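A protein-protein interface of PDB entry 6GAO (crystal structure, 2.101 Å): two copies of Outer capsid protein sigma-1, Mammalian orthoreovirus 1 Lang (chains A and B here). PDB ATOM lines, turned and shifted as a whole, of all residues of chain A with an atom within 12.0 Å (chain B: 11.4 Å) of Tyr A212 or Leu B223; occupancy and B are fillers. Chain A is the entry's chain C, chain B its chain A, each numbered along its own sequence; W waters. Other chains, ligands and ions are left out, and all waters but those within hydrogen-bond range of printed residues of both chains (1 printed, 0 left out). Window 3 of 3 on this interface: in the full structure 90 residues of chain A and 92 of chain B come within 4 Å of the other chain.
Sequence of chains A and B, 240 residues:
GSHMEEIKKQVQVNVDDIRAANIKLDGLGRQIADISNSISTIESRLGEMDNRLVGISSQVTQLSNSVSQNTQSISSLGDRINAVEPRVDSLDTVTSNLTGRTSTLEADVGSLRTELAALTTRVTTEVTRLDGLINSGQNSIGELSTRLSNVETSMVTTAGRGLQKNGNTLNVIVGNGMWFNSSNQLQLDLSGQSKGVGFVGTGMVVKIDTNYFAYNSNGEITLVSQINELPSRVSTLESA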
ATOM      1  N   GLY A 196      12.302   9.325 -28.643  1.00  0.00           N
ATOM      2  CA  GLY A 196      11.553  10.089 -27.688  1.00  0.00           C
ATOM      3  C   GLY A 196      12.380  10.718 -26.596  1.00  0.00           C
ATOM      4  O   GLY A 196      11.840  11.551 -25.855  1.00  0.00           O
ATOM      5  N   VAL A 206      12.359  14.939 -22.977  1.00  0.00           N
ATOM      6  CA  VAL A 206      11.445  14.039 -23.676  1.00  0.00           C
ATOM      7  C   VAL A 206      11.071  14.750 -24.963  1.00  0.00           C
ATOM      8  O   VAL A 206      10.438  15.811 -24.933  1.00  0.00           O
ATOM      9  CB  VAL A 206      10.195  13.704 -22.849  1.00  0.00           C
ATOM     10  CG1 VAL A 206       9.175  12.975 -23.710  1.00  0.00           C
ATOM     11  CG2 VAL A 206      10.555  12.837 -21.631  1.00  0.00           C
ATOM     12  N   LYS A 207      11.489  14.197 -26.095  1.00  0.00           N
ATOM     13  CA  LYS A 207      11.197  14.849 -27.363  1.00  0.00           C
ATOM     14  C   LYS A 207       9.714  14.684 -27.701  1.00  0.00           C
ATOM     15  O   LYS A 207       9.171  13.578 -27.595  1.00  0.00           O
ATOM     16  CB  LYS A 207      12.095  14.263 -28.445  1.00  0.00           C
ATOM     17  CG  LYS A 207      13.569  14.422 -28.140  1.00  0.00           C
ATOM     18  CD  LYS A 207      14.439  13.792 -29.243  1.00  0.00           C
ATOM     19  CE  LYS A 207      14.210  14.391 -30.602  1.00  0.00           C
ATOM     20  NZ  LYS A 207      15.335  14.153 -31.533  1.00  0.00           N
ATOM     21  N   ILE A 208       9.039  15.788 -28.060  1.00  0.00           N
ATOM     22  CA  ILE A 208       7.583  15.787 -28.177  1.00  0.00           C
ATOM     23  C   ILE A 208       7.148  16.504 -29.450  1.00  0.00           C
ATOM     24  O   ILE A 208       7.674  17.566 -29.800  1.00  0.00           O
ATOM     25  CB  ILE A 208       6.860  16.428 -26.954  1.00  0.00           C
ATOM     26  CG1 ILE A 208       7.427  17.797 -26.550  1.00  0.00           C
ATOM     27  CG2 ILE A 208       6.778  15.503 -25.771  1.00  0.00           C
ATOM     28  CD1 ILE A 208       6.443  18.602 -25.683  1.00  0.00           C
ATOM     29  N   ASP A 209       6.172  15.916 -30.132  1.00  0.00           N
ATOM     30  CA  ASP A 209       5.480  16.578 -31.228  1.00  0.00           C
ATOM     31  C   ASP A 209       4.655  17.712 -30.635  1.00  0.00           C
ATOM     32  O   ASP A 209       3.658  17.468 -29.941  1.00  0.00           O
ATOM     33  CB  ASP A 209       4.608  15.560 -31.951  1.00  0.00           C
ATOM     34  CG  ASP A 209       3.882  16.151 -33.139  1.00  0.00           C
ATOM     35  OD1 ASP A 209       3.692  17.374 -33.189  1.00  0.00           O
ATOM     36  OD2 ASP A 209       3.485  15.386 -34.014  1.00  0.00           O
ATOM     37  N   THR A 210       5.086  18.949 -30.857  1.00  0.00           N
ATOM     38  CA  THR A 210       4.412  20.076 -30.216  1.00  0.00           C
ATOM     39  C   THR A 210       3.086  20.441 -30.877  1.00  0.00           C
ATOM     40  O   THR A 210       2.485  21.445 -30.498  1.00  0.00           O
ATOM     41  CB  THR A 210       5.311  21.310 -30.188  1.00  0.00           C
ATOM     42  OG1 THR A 210       5.632  21.701 -31.523  1.00  0.00           O
ATOM     43  CG2 THR A 210       6.611  21.028 -29.405  1.00  0.00           C
ATOM     44  N   ASN A 211       2.623  19.672 -31.857  1.00  0.00           N
ATOM     45  CA  ASN A 211       1.249  19.781 -32.325  1.00  0.00           C
ATOM     46  C   ASN A 211       0.264  19.092 -31.395  1.00  0.00           C
ATOM     47  O   ASN A 211      -0.949  19.283 -31.544  1.00  0.00           O
ATOM     48  CB  ASN A 211       1.111  19.157 -33.703  1.00  0.00           C
ATOM     49  CG  ASN A 211       1.744  19.982 -34.775  1.00  0.00           C
ATOM     50  OD1 ASN A 211       1.831  21.213 -34.672  1.00  0.00           O
ATOM     51  ND2 ASN A 211       2.192  19.315 -35.829  1.00  0.00           N
ATOM     52  N   TYR A 212       0.751  18.278 -30.462  1.00  0.00           N
ATOM     53  CA  TYR A 212      -0.138  17.531 -29.586  1.00  0.00           C
ATOM     54  C   TYR A 212       0.230  17.715 -28.121  1.00  0.00           C
ATOM     55  O   TYR A 212      -0.652  17.721 -27.261  1.00  0.00           O
ATOM     56  CB  TYR A 212      -0.101  16.049 -29.934  1.00  0.00           C
ATOM     57  CG  TYR A 212      -0.553  15.721 -31.334  1.00  0.00           C
ATOM     58  CD1 TYR A 212      -1.847  16.012 -31.761  1.00  0.00           C
ATOM     59  CD2 TYR A 212       0.302  15.101 -32.222  1.00  0.00           C
ATOM     60  CE1 TYR A 212      -2.263  15.701 -33.054  1.00  0.00           C
ATOM     61  CE2 TYR A 212      -0.100  14.784 -33.496  1.00  0.00           C
ATOM     62  CZ  TYR A 212      -1.379  15.081 -33.915  1.00  0.00           C
ATOM     63  OH  TYR A 212      -1.747  14.744 -35.199  1.00  0.00           O
ATOM     64  N   PHE A 213       1.520  17.873 -27.822  1.00  0.00           N
ATOM     65  CA  PHE A 213       2.007  17.879 -26.454  1.00  0.00           C
ATOM     66  C   PHE A 213       2.669  19.202 -26.110  1.00  0.00           C
ATOM     67  O   PHE A 213       3.117  19.943 -26.987  1.00  0.00           O
ATOM     68  CB  PHE A 213       3.014  16.741 -26.243  1.00  0.00           C
ATOM     69  CG  PHE A 213       2.498  15.400 -26.692  1.00  0.00           C
ATOM     70  CD1 PHE A 213       1.349  14.869 -26.127  1.00  0.00           C
ATOM     71  CD2 PHE A 213       3.150  14.687 -27.684  1.00  0.00           C
ATOM     72  CE1 PHE A 213       0.876  13.660 -26.526  1.00  0.00           C
ATOM     73  CE2 PHE A 213       2.688  13.477 -28.081  1.00  0.00           C
ATOM     74  CZ  PHE A 213       1.541  12.954 -27.511  1.00  0.00           C
ATOM     75  N   ALA A 214       2.733  19.487 -24.812  1.00  0.00           N
ATOM     76  CA  ALA A 214       3.637  20.504 -24.297  1.00  0.00           C
ATOM     77  C   ALA A 214       4.121  20.085 -22.913  1.00  0.00           C
ATOM     78  O   ALA A 214       3.731  19.040 -22.369  1.00  0.00           O
ATOM     79  CB  ALA A 214       2.978  21.889 -24.245  1.00  0.00           C
ATOM     80  N   TYR A 215       4.963  20.925 -22.338  1.00  0.00           N
ATOM     81  CA  TYR A 215       5.412  20.771 -20.965  1.00  0.00           C
ATOM     82  C   TYR A 215       4.721  21.815 -20.098  1.00  0.00           C
ATOM     83  O   TYR A 215       4.812  23.009 -20.384  1.00  0.00           O
ATOM     84  CB  TYR A 215       6.921  20.971 -20.841  1.00  0.00           C
ATOM     85  CG  TYR A 215       7.850  20.295 -21.835  1.00  0.00           C
ATOM     86  CD1 TYR A 215       8.068  18.910 -21.810  1.00  0.00           C
ATOM     87  CD2 TYR A 215       8.595  21.058 -22.725  1.00  0.00           C
ATOM     88  CE1 TYR A 215       8.969  18.295 -22.694  1.00  0.00           C
ATOM     89  CE2 TYR A 215       9.503  20.460 -23.601  1.00  0.00           C
ATOM     90  CZ  TYR A 215       9.684  19.079 -23.574  1.00  0.00           C
ATOM     91  OH  TYR A 215      10.574  18.509 -24.452  1.00  0.00           O
ATOM     92  N   ASN A 216       4.080  21.384 -19.017  1.00  0.00           N
ATOM     93  CA  ASN A 216       3.439  22.338 -18.118  1.00  0.00           C
ATOM     94  C   ASN A 216       4.468  22.916 -17.138  1.00  0.00           C
ATOM     95  O   ASN A 216       5.674  22.666 -17.241  1.00  0.00           O
ATOM     96  CB  ASN A 216       2.250  21.686 -17.422  1.00  0.00           C
ATOM     97  CG  ASN A 216       2.642  20.525 -16.539  1.00  0.00           C
ATOM     98  OD1 ASN A 216       3.674  20.550 -15.864  1.00  0.00           O
ATOM     99  ND2 ASN A 216       1.797  19.502 -16.515  1.00  0.00           N
ATOM    100  N   GLU A 220       5.872  18.389 -16.516  1.00  0.00           N
ATOM    101  CA  GLU A 220       5.350  17.126 -17.026  1.00  0.00           C
ATOM    102  C   GLU A 220       4.859  17.269 -18.459  1.00  0.00           C
ATOM    103  O   GLU A 220       4.628  18.379 -18.951  1.00  0.00           O
ATOM    104  CB  GLU A 220       4.222  16.618 -16.138  1.00  0.00           C
ATOM    105  CG  GLU A 220       4.364  17.003 -14.663  1.00  0.00           C
ATOM    106  CD  GLU A 220       3.055  16.848 -13.888  1.00  0.00           C
ATOM    107  OE1 GLU A 220       2.007  17.344 -14.354  1.00  0.00           O
ATOM    108  OE2 GLU A 220       3.080  16.206 -12.822  1.00  0.00           O
ATOM    109  N   ILE A 221       4.688  16.130 -19.136  1.00  0.00           N
ATOM    110  CA  ILE A 221       4.153  16.144 -20.497  1.00  0.00           C
ATOM    111  C   ILE A 221       2.635  16.199 -20.431  1.00  0.00           C
ATOM    112  O   ILE A 221       2.011  15.449 -19.673  1.00  0.00           O
ATOM    113  CB  ILE A 221       4.613  14.924 -21.316  1.00  0.00           C
ATOM    114  CG1 ILE A 221       6.082  15.041 -21.727  1.00  0.00           C
ATOM    115  CG2 ILE A 221       3.806  14.857 -22.598  1.00  0.00           C
ATOM    116  CD1 ILE A 221       7.002  14.306 -20.810  1.00  0.00           C
ATOM    117  N   THR A 222       2.033  17.065 -21.240  1.00  0.00           N
ATOM    118  CA  THR A 222       0.588  17.204 -21.233  1.00  0.00           C
ATOM    119  C   THR A 222       0.092  17.415 -22.654  1.00  0.00           C
ATOM    120  O   THR A 222       0.868  17.701 -23.571  1.00  0.00           O
ATOM    121  CB  THR A 222       0.142  18.358 -20.326  1.00  0.00           C
ATOM    122  OG1 THR A 222      -1.287  18.362 -20.238  1.00  0.00           O
ATOM    123  CG2 THR A 222       0.632  19.683 -20.862  1.00  0.00           C
ATOM    124  N   LEU A 223      -1.215  17.258 -22.836  1.00  0.00           N
ATOM    125  CA  LEU A 223      -1.851  17.612 -24.102  1.00  0.00           C
ATOM    126  C   LEU A 223      -2.049  19.119 -24.195  1.00  0.00           C
ATOM    127  O   LEU A 223      -2.315  19.781 -23.191  1.00  0.00           O
ATOM    128  CB  LEU A 223      -3.190  16.885 -24.258  1.00  0.00           C
ATOM    129  CG  LEU A 223      -3.093  15.348 -24.192  1.00  0.00           C
ATOM    130  CD1 LEU A 223      -4.460  14.694 -24.143  1.00  0.00           C
ATOM    131  CD2 LEU A 223      -2.319  14.798 -25.375  1.00  0.00           C
ATOM    132  N   VAL A 224      -1.866  19.661 -25.398  1.00  0.00           N
ATOM    133  CA  VAL A 224      -2.068  21.093 -25.666  1.00  0.00           C
ATOM    134  C   VAL A 224      -3.550  21.501 -25.601  1.00  0.00           C
ATOM    135  O   VAL A 224      -4.446  20.759 -26.024  1.00  0.00           O
ATOM    136  CB  VAL A 224      -1.482  21.482 -27.041  1.00  0.00           C
ATOM    137  CG1 VAL A 224      -0.075  20.970 -27.168  1.00  0.00           C
ATOM    138  CG2 VAL A 224      -2.353  20.936 -28.178  1.00  0.00           C
ATOM    139  N   LYS B 207       9.116   4.650 -23.454  1.00  0.00           N
ATOM    140  CA  LYS B 207       8.240   3.528 -23.738  1.00  0.00           C
ATOM    141  C   LYS B 207       6.843   4.064 -24.026  1.00  0.00           C
ATOM    142  O   LYS B 207       6.311   4.847 -23.237  1.00  0.00           O
ATOM    143  CB  LYS B 207       8.240   2.559 -22.558  1.00  0.00           C
ATOM    144  CG  LYS B 207       9.634   1.985 -22.270  1.00  0.00           C
ATOM    145  CD  LYS B 207       9.626   1.133 -21.009  1.00  0.00           C
ATOM    146  CE  LYS B 207       8.720  -0.131 -21.180  1.00  0.00           C
ATOM    147  NZ  LYS B 207       9.162  -1.149 -20.122  1.00  0.00           N
ATOM    148  N   ILE B 208       6.270   3.662 -25.162  1.00  0.00           N
ATOM    149  CA  ILE B 208       4.993   4.198 -25.655  1.00  0.00           C
ATOM    150  C   ILE B 208       4.021   3.072 -25.970  1.00  0.00           C
ATOM    151  O   ILE B 208       4.397   2.037 -26.533  1.00  0.00           O
ATOM    152  CB  ILE B 208       5.167   5.043 -26.928  1.00  0.00           C
ATOM    153  CG1 ILE B 208       5.995   4.259 -27.945  1.00  0.00           C
ATOM    154  CG2 ILE B 208       5.750   6.435 -26.638  1.00  0.00           C
ATOM    155  CD1 ILE B 208       6.188   5.017 -29.231  1.00  0.00           C
ATOM    156  N   ASP B 209       2.761   3.292 -25.629  1.00  0.00           N
ATOM    157  CA  ASP B 209       1.677   2.426 -26.069  1.00  0.00           C
ATOM    158  C   ASP B 209       1.442   2.657 -27.557  1.00  0.00           C
ATOM    159  O   ASP B 209       0.962   3.719 -27.967  1.00  0.00           O
ATOM    160  CB  ASP B 209       0.416   2.731 -25.262  1.00  0.00           C
ATOM    161  CG  ASP B 209      -0.693   1.706 -25.484  1.00  0.00           C
ATOM    162  OD1 ASP B 209      -0.854   1.181 -26.615  1.00  0.00           O
ATOM    163  OD2 ASP B 209      -1.408   1.432 -24.504  1.00  0.00           O
ATOM    164  N   THR B 210       1.781   1.685 -28.379  1.00  0.00           N
ATOM    165  CA  THR B 210       1.669   1.938 -29.801  1.00  0.00           C
ATOM    166  C   THR B 210       0.240   1.812 -30.306  1.00  0.00           C
ATOM    167  O   THR B 210       0.039   1.750 -31.514  1.00  0.00           O
ATOM    168  CB  THR B 210       2.615   1.023 -30.578  1.00  0.00           C
ATOM    169  OG1 THR B 210       2.628  -0.275 -29.996  1.00  0.00           O
ATOM    170  CG2 THR B 210       4.011   1.588 -30.572  1.00  0.00           C
ATOM    171  N   ASN B 211      -0.758   1.795 -29.415  1.00  0.00           N
ATOM    172  CA  ASN B 211      -2.125   2.026 -29.853  1.00  0.00           C
ATOM    173  C   ASN B 211      -2.391   3.501 -30.057  1.00  0.00           C
ATOM    174  O   ASN B 211      -3.284   3.876 -30.830  1.00  0.00           O
ATOM    175  CB  ASN B 211      -3.124   1.509 -28.823  1.00  0.00           C
ATOM    176  CG  ASN B 211      -3.208   0.035 -28.810  1.00  0.00           C
ATOM    177  OD1 ASN B 211      -2.964  -0.603 -29.830  1.00  0.00           O
ATOM    178  ND2 ASN B 211      -3.540  -0.538 -27.651  1.00  0.00           N
ATOM    179  N   TYR B 212      -1.655   4.340 -29.343  1.00  0.00           N
ATOM    180  CA  TYR B 212      -1.954   5.755 -29.276  1.00  0.00           C
ATOM    181  C   TYR B 212      -0.781   6.627 -29.628  1.00  0.00           C
ATOM    182  O   TYR B 212      -0.999   7.758 -30.071  1.00  0.00           O
ATOM    183  CB  TYR B 212      -2.448   6.121 -27.873  1.00  0.00           C
ATOM    184  CG  TYR B 212      -3.603   5.245 -27.450  1.00  0.00           C
ATOM    185  CD1 TYR B 212      -4.836   5.333 -28.103  1.00  0.00           C
ATOM    186  CD2 TYR B 212      -3.459   4.303 -26.433  1.00  0.00           C
ATOM    187  CE1 TYR B 212      -5.900   4.521 -27.742  1.00  0.00           C
ATOM    188  CE2 TYR B 212      -4.514   3.488 -26.068  1.00  0.00           C
ATOM    189  CZ  TYR B 212      -5.738   3.606 -26.725  1.00  0.00           C
ATOM    190  OH  TYR B 212      -6.803   2.810 -26.365  1.00  0.00           O
ATOM    191  N   PHE B 213       0.450   6.130 -29.476  1.00  0.00           N
ATOM    192  CA  PHE B 213       1.641   6.901 -29.772  1.00  0.00           C
ATOM    193  C   PHE B 213       2.488   6.206 -30.826  1.00  0.00           C
ATOM    194  O   PHE B 213       2.441   4.986 -31.005  1.00  0.00           O
ATOM    195  CB  PHE B 213       2.501   7.110 -28.527  1.00  0.00           C
ATOM    196  CG  PHE B 213       1.751   7.619 -27.349  1.00  0.00           C
ATOM    197  CD1 PHE B 213       1.454   8.962 -27.234  1.00  0.00           C
ATOM    198  CD2 PHE B 213       1.362   6.752 -26.337  1.00  0.00           C
ATOM    199  CE1 PHE B 213       0.757   9.434 -26.130  1.00  0.00           C
ATOM    200  CE2 PHE B 213       0.674   7.209 -25.232  1.00  0.00           C
ATOM    201  CZ  PHE B 213       0.374   8.558 -25.123  1.00  0.00           C
ATOM    202  N   ALA B 214       3.293   7.021 -31.497  1.00  0.00           N
ATOM    203  CA  ALA B 214       4.380   6.555 -32.331  1.00  0.00           C
ATOM    204  C   ALA B 214       5.540   7.535 -32.177  1.00  0.00           C
ATOM    205  O   ALA B 214       5.437   8.571 -31.506  1.00  0.00           O
ATOM    206  CB  ALA B 214       3.930   6.417 -33.800  1.00  0.00           C
ATOM    207  N   TYR B 215       6.664   7.192 -32.777  1.00  0.00           N
ATOM    208  CA  TYR B 215       7.772   8.130 -32.912  1.00  0.00           C
ATOM    209  C   TYR B 215       7.735   8.704 -34.310  1.00  0.00           C
ATOM    210  O   TYR B 215       7.525   7.971 -35.273  1.00  0.00           O
ATOM    211  CB  TYR B 215       9.109   7.460 -32.708  1.00  0.00           C
ATOM    212  CG  TYR B 215       9.231   6.605 -31.479  1.00  0.00           C
ATOM    213  CD1 TYR B 215       9.364   7.182 -30.199  1.00  0.00           C
ATOM    214  CD2 TYR B 215       9.300   5.228 -31.596  1.00  0.00           C
ATOM    215  CE1 TYR B 215       9.521   6.396 -29.084  1.00  0.00           C
ATOM    216  CE2 TYR B 215       9.447   4.439 -30.497  1.00  0.00           C
ATOM    217  CZ  TYR B 215       9.578   5.030 -29.243  1.00  0.00           C
ATOM    218  OH  TYR B 215       9.719   4.223 -28.163  1.00  0.00           O
ATOM    219  N   ASN B 216       7.939   9.998 -34.432  1.00  0.00           N
ATOM    220  CA  ASN B 216       7.905  10.543 -35.774  1.00  0.00           C
ATOM    221  C   ASN B 216       9.326  10.605 -36.342  1.00  0.00           C
ATOM    222  O   ASN B 216      10.317  10.178 -35.717  1.00  0.00           O
ATOM    223  CB  ASN B 216       7.203  11.912 -35.791  1.00  0.00           C
ATOM    224  CG  ASN B 216       7.951  12.976 -35.001  1.00  0.00           C
ATOM    225  OD1 ASN B 216       9.175  12.885 -34.786  1.00  0.00           O
ATOM    226  ND2 ASN B 216       7.220  13.986 -34.545  1.00  0.00           N
ATOM    227  N   SER B 217       9.435  11.191 -37.534  1.00  0.00           N
ATOM    228  CA  SER B 217      10.745  11.264 -38.176  1.00  0.00           C
ATOM    229  C   SER B 217      11.701  12.235 -37.490  1.00  0.00           C
ATOM    230  O   SER B 217      12.876  12.277 -37.868  1.00  0.00           O
ATOM    231  CB  SER B 217      10.583  11.677 -39.637  1.00  0.00           C
ATOM    232  OG  SER B 217      10.303  13.075 -39.668  1.00  0.00           O
ATOM    233  N   ASN B 218      11.239  13.030 -36.523  1.00  0.00           N
ATOM    234  CA  ASN B 218      12.149  13.871 -35.754  1.00  0.00           C
ATOM    235  C   ASN B 218      12.609  13.206 -34.470  1.00  0.00           C
ATOM    236  O   ASN B 218      13.292  13.850 -33.679  1.00  0.00           O
ATOM    237  CB  ASN B 218      11.509  15.205 -35.364  1.00  0.00           C
ATOM    238  CG  ASN B 218      11.533  16.217 -36.473  1.00  0.00           C
ATOM    239  OD1 ASN B 218      10.479  16.685 -36.917  1.00  0.00           O
ATOM    240  ND2 ASN B 218      12.726  16.584 -36.917  1.00  0.00           N
ATOM    241  N   GLY B 219      12.208  11.965 -34.229  1.00  0.00           N
ATOM    242  CA  GLY B 219      12.463  11.314 -32.969  1.00  0.00           C
ATOM    243  C   GLY B 219      11.561  11.741 -31.831  1.00  0.00           C
ATOM    244  O   GLY B 219      11.801  11.330 -30.689  1.00  0.00           O
ATOM    245  N   GLU B 220      10.551  12.556 -32.093  1.00  0.00           N
ATOM    246  CA  GLU B 220       9.612  12.979 -31.067  1.00  0.00           C
ATOM    247  C   GLU B 220       8.513  11.941 -30.899  1.00  0.00           C
ATOM    248  O   GLU B 220       8.244  11.148 -31.804  1.00  0.00           O
ATOM    249  CB  GLU B 220       9.001  14.323 -31.438  1.00  0.00           C
ATOM    250  CG  GLU B 220      10.029  15.419 -31.654  1.00  0.00           C
ATOM    251  CD  GLU B 220       9.488  16.526 -32.500  1.00  0.00           C
ATOM    252  OE1 GLU B 220       8.481  16.273 -33.174  1.00  0.00           O
ATOM    253  OE2 GLU B 220      10.068  17.622 -32.515  1.00  0.00           O
ATOM    254  N   ILE B 221       7.894  11.915 -29.721  1.00  0.00           N
ATOM    255  CA  ILE B 221       6.698  11.101 -29.583  1.00  0.00           C
ATOM    256  C   ILE B 221       5.542  11.879 -30.195  1.00  0.00           C
ATOM    257  O   ILE B 221       5.477  13.110 -30.075  1.00  0.00           O
ATOM    258  CB  ILE B 221       6.408  10.735 -28.121  1.00  0.00           C
ATOM    259  CG1 ILE B 221       6.269  12.003 -27.266  1.00  0.00           C
ATOM    260  CG2 ILE B 221       7.458   9.763 -27.593  1.00  0.00           C
ATOM    261  CD1 ILE B 221       5.649  11.735 -25.927  1.00  0.00           C
ATOM    262  N   THR B 222       4.657  11.167 -30.881  1.00  0.00           N
ATOM    263  CA  THR B 222       3.507  11.772 -31.541  1.00  0.00           C
ATOM    264  C   THR B 222       2.287  10.872 -31.348  1.00  0.00           C
ATOM    265  O   THR B 222       2.389   9.771 -30.810  1.00  0.00           O
ATOM    266  CB  THR B 222       3.813  12.010 -33.032  1.00  0.00           C
ATOM    267  OG1 THR B 222       2.743  12.738 -33.646  1.00  0.00           O
ATOM    268  CG2 THR B 222       4.057  10.663 -33.773  1.00  0.00           C
ATOM    269  N   LEU B 223       1.111  11.353 -31.776  1.00  0.00           N
ATOM    270  CA  LEU B 223      -0.141  10.602 -31.645  1.00  0.00           C
ATOM    271  C   LEU B 223      -0.518   9.965 -32.974  1.00  0.00           C
ATOM    272  O   LEU B 223      -0.293  10.557 -34.035  1.00  0.00           O
ATOM    273  CB  LEU B 223      -1.287  11.495 -31.182  1.00  0.00           C
ATOM    274  CG  LEU B 223      -1.124  12.053 -29.777  1.00  0.00           C
ATOM    275  CD1 LEU B 223      -2.066  13.203 -29.597  1.00  0.00           C
ATOM    276  CD2 LEU B 223      -1.406  10.968 -28.760  1.00  0.00           C
ATOM    277  N   VAL B 224      -1.082   8.760 -32.917  1.00  0.00           N
ATOM    278  CA  VAL B 224      -1.518   8.060 -34.124  1.00  0.00           C
ATOM    279  C   VAL B 224      -3.033   8.118 -34.208  1.00  0.00           C
ATOM    280  O   VAL B 224      -3.725   8.216 -33.189  1.00  0.00           O
ATOM    281  CB  VAL B 224      -1.043   6.591 -34.182  1.00  0.00           C
ATOM    282  CG1 VAL B 224       0.371   6.510 -34.693  1.00  0.00           C
ATOM    283  CG2 VAL B 224      -1.162   5.948 -32.826  1.00  0.00           C
ATOM    284  N   SER B 225      -3.542   8.056 -35.445  1.00  0.00           N
ATOM    285  CA  SER B 225      -4.983   8.065 -35.775  1.00  0.00           C
ATOM    286  C   SER B 225      -5.863   8.867 -34.825  1.00  0.00           C
ATOM    287  O   SER B 225      -6.433   8.301 -33.888  1.00  0.00           O
ATOM    288  CB  SER B 225      -5.510   6.628 -35.844  1.00  0.00           C
ATOM    289  OG  SER B 225      -5.405   5.979 -34.590  1.00  0.00           O
HETATM  290  O   HOH W   1       7.234  18.695 -32.933  1.00  0.00           O
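Printed residues of chain B within 4 Å of Gly A196: Tyr B215 (3.96 Å) and Gly B219 (2.9 Å).
Val A206 touches none of the printed residues of chain B.
Printed residues of chain B within 4 Å of Asp A209: Glu B220, Ile B221 and Thr B222.
No residue of chain B comes within 4 Å of Thr A210.
No residue of chain B comes within 4 Å of Asn A211.
Printed residues of chain B within 4 Å of Tyr A212: Thr B222 and Leu B223.
Phe A213 touches four residues of chain B.
No residue of chain B comes within 4 Å of Thr A222.
Of chain A, only Phe A213 (3.9 Å) comes within 4 Å of Phe B213.
Of the printed residues of chain A, Tyr B215 touches Gly A196 (3.96 Å).
Ser B217 touches none of the printed residues of chain A.
Printed residues of chain A within 4 Å of Gly B219: Gly A196 and Lys A207.
Of chain A, only Lys A207 (3.0 Å), Ile A208 (3.8 Å), Asp A209 (2.9 Å) and Phe A213 (3.4 Å) come within 4 Å of Ile B221.
Printed residues of chain A within 4 Å of Thr B222: Asp A209 (2.8 Å), Tyr A212 (3.5 Å) and Phe A213 (3.9 Å).
Leu B223 touches just these residues of chain A: Tyr A212 (3.4 Å) and Phe A213 (3.6 Å).
No residue of chain A comes within 4 Å of Ser B225.
The nearest residue of chain B that does not touch Tyr A212 is Ile B221 (5.9 Å).
Hydrophobic or aromatic side chains of chain A within 4 Å of the printed part of chain B: Ile A208, Tyr A212 and Phe A213.
N of Thr B222 sits at hydrogen-bond distance from O of Ala B214.
The backbone NH of Asn B218 is in hydrogen-bond range of the side-chain amide oxygen of Asn B216, at 2.7 Å.
The side-chain amide oxygen of Asn B216 lies within hydrogen-bond range of the backbone NH of Gly B219.
The side-chain amide nitrogen (ND2) of Asn B216 lies within hydrogen-bond range of the side-chain carboxylate (OE1) of Glu B220 (2.9 Å).
N of Lys A207 sits at hydrogen-bond distance from O of Gly A196.
The backbone NH of Val A224 lies within hydrogen-bond range of the backbone carbonyl oxygen of Tyr A212, 3.0 Å away.
Water W1 lies within hydrogen-bond range of OE1 of Glu B220 (2.7 Å), N of Thr A210 (3.0 Å) and O of Ile A208 (3.4 Å).
The side-chain amino group (NZ) of Lys A207 is in hydrogen-bond range of the backbone carbonyl oxygen (O) of Asn B218 (3.0 Å).
The backbone NH (N) of Gly A196 lies within hydrogen-bond range of the backbone carbonyl oxygen (O) of Gly B219 (2.9 Å).
The backbone NH of Ile B221 is in hydrogen-bond range of the backbone carbonyl oxygen of Lys A207 (3.0 Å).
O of Ile B221 sits at hydrogen-bond distance from N of Asp A209 (2.9 Å).
The side-chain hydroxyl (OG1) of Thr B222 sits at hydrogen-bond distance from the side-chain carboxylate (OD2) of Asp A209 (2.8 Å).
Lys A207 touches Glu B220, but with the chains exchanged Glu A220 does not touch Lys B207 (13.4 Å).
Lys A207 touches Ile B221, but with the chains exchanged Ile A221 does not touch Lys B207 (9.8 Å).
Ile A208 touches Ile B221, but with the chains exchanged Ile A221 does not touch Ile B208 (9.5 Å).
Phe A213 touches its own counterpart, Phe B213.
15 positions are printed for both chains.
Gly A196 touches Tyr B215 (N to CD1, 3.96 Å).
O of Lys A207 touches CA of Glu B220, at 3.6 Å.
O of Ile A208 touches CD of Glu B220 (3.4 Å).
Ile A208 touches Ile B221.
Asp A209 touches Glu B220 (N to CB, 3.5 Å).
OG1 of Thr B222 touches CE2 of Tyr A212, at 3.5 Å.
Leu B223 touches Tyr A212 (CD1 to CG, 3.4 Å).
Phe A213 touches Phe B213.
Ile B221 touches Phe A213.
Phe A213 touches Thr B222 (CE2 to CA, 3.9 Å).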
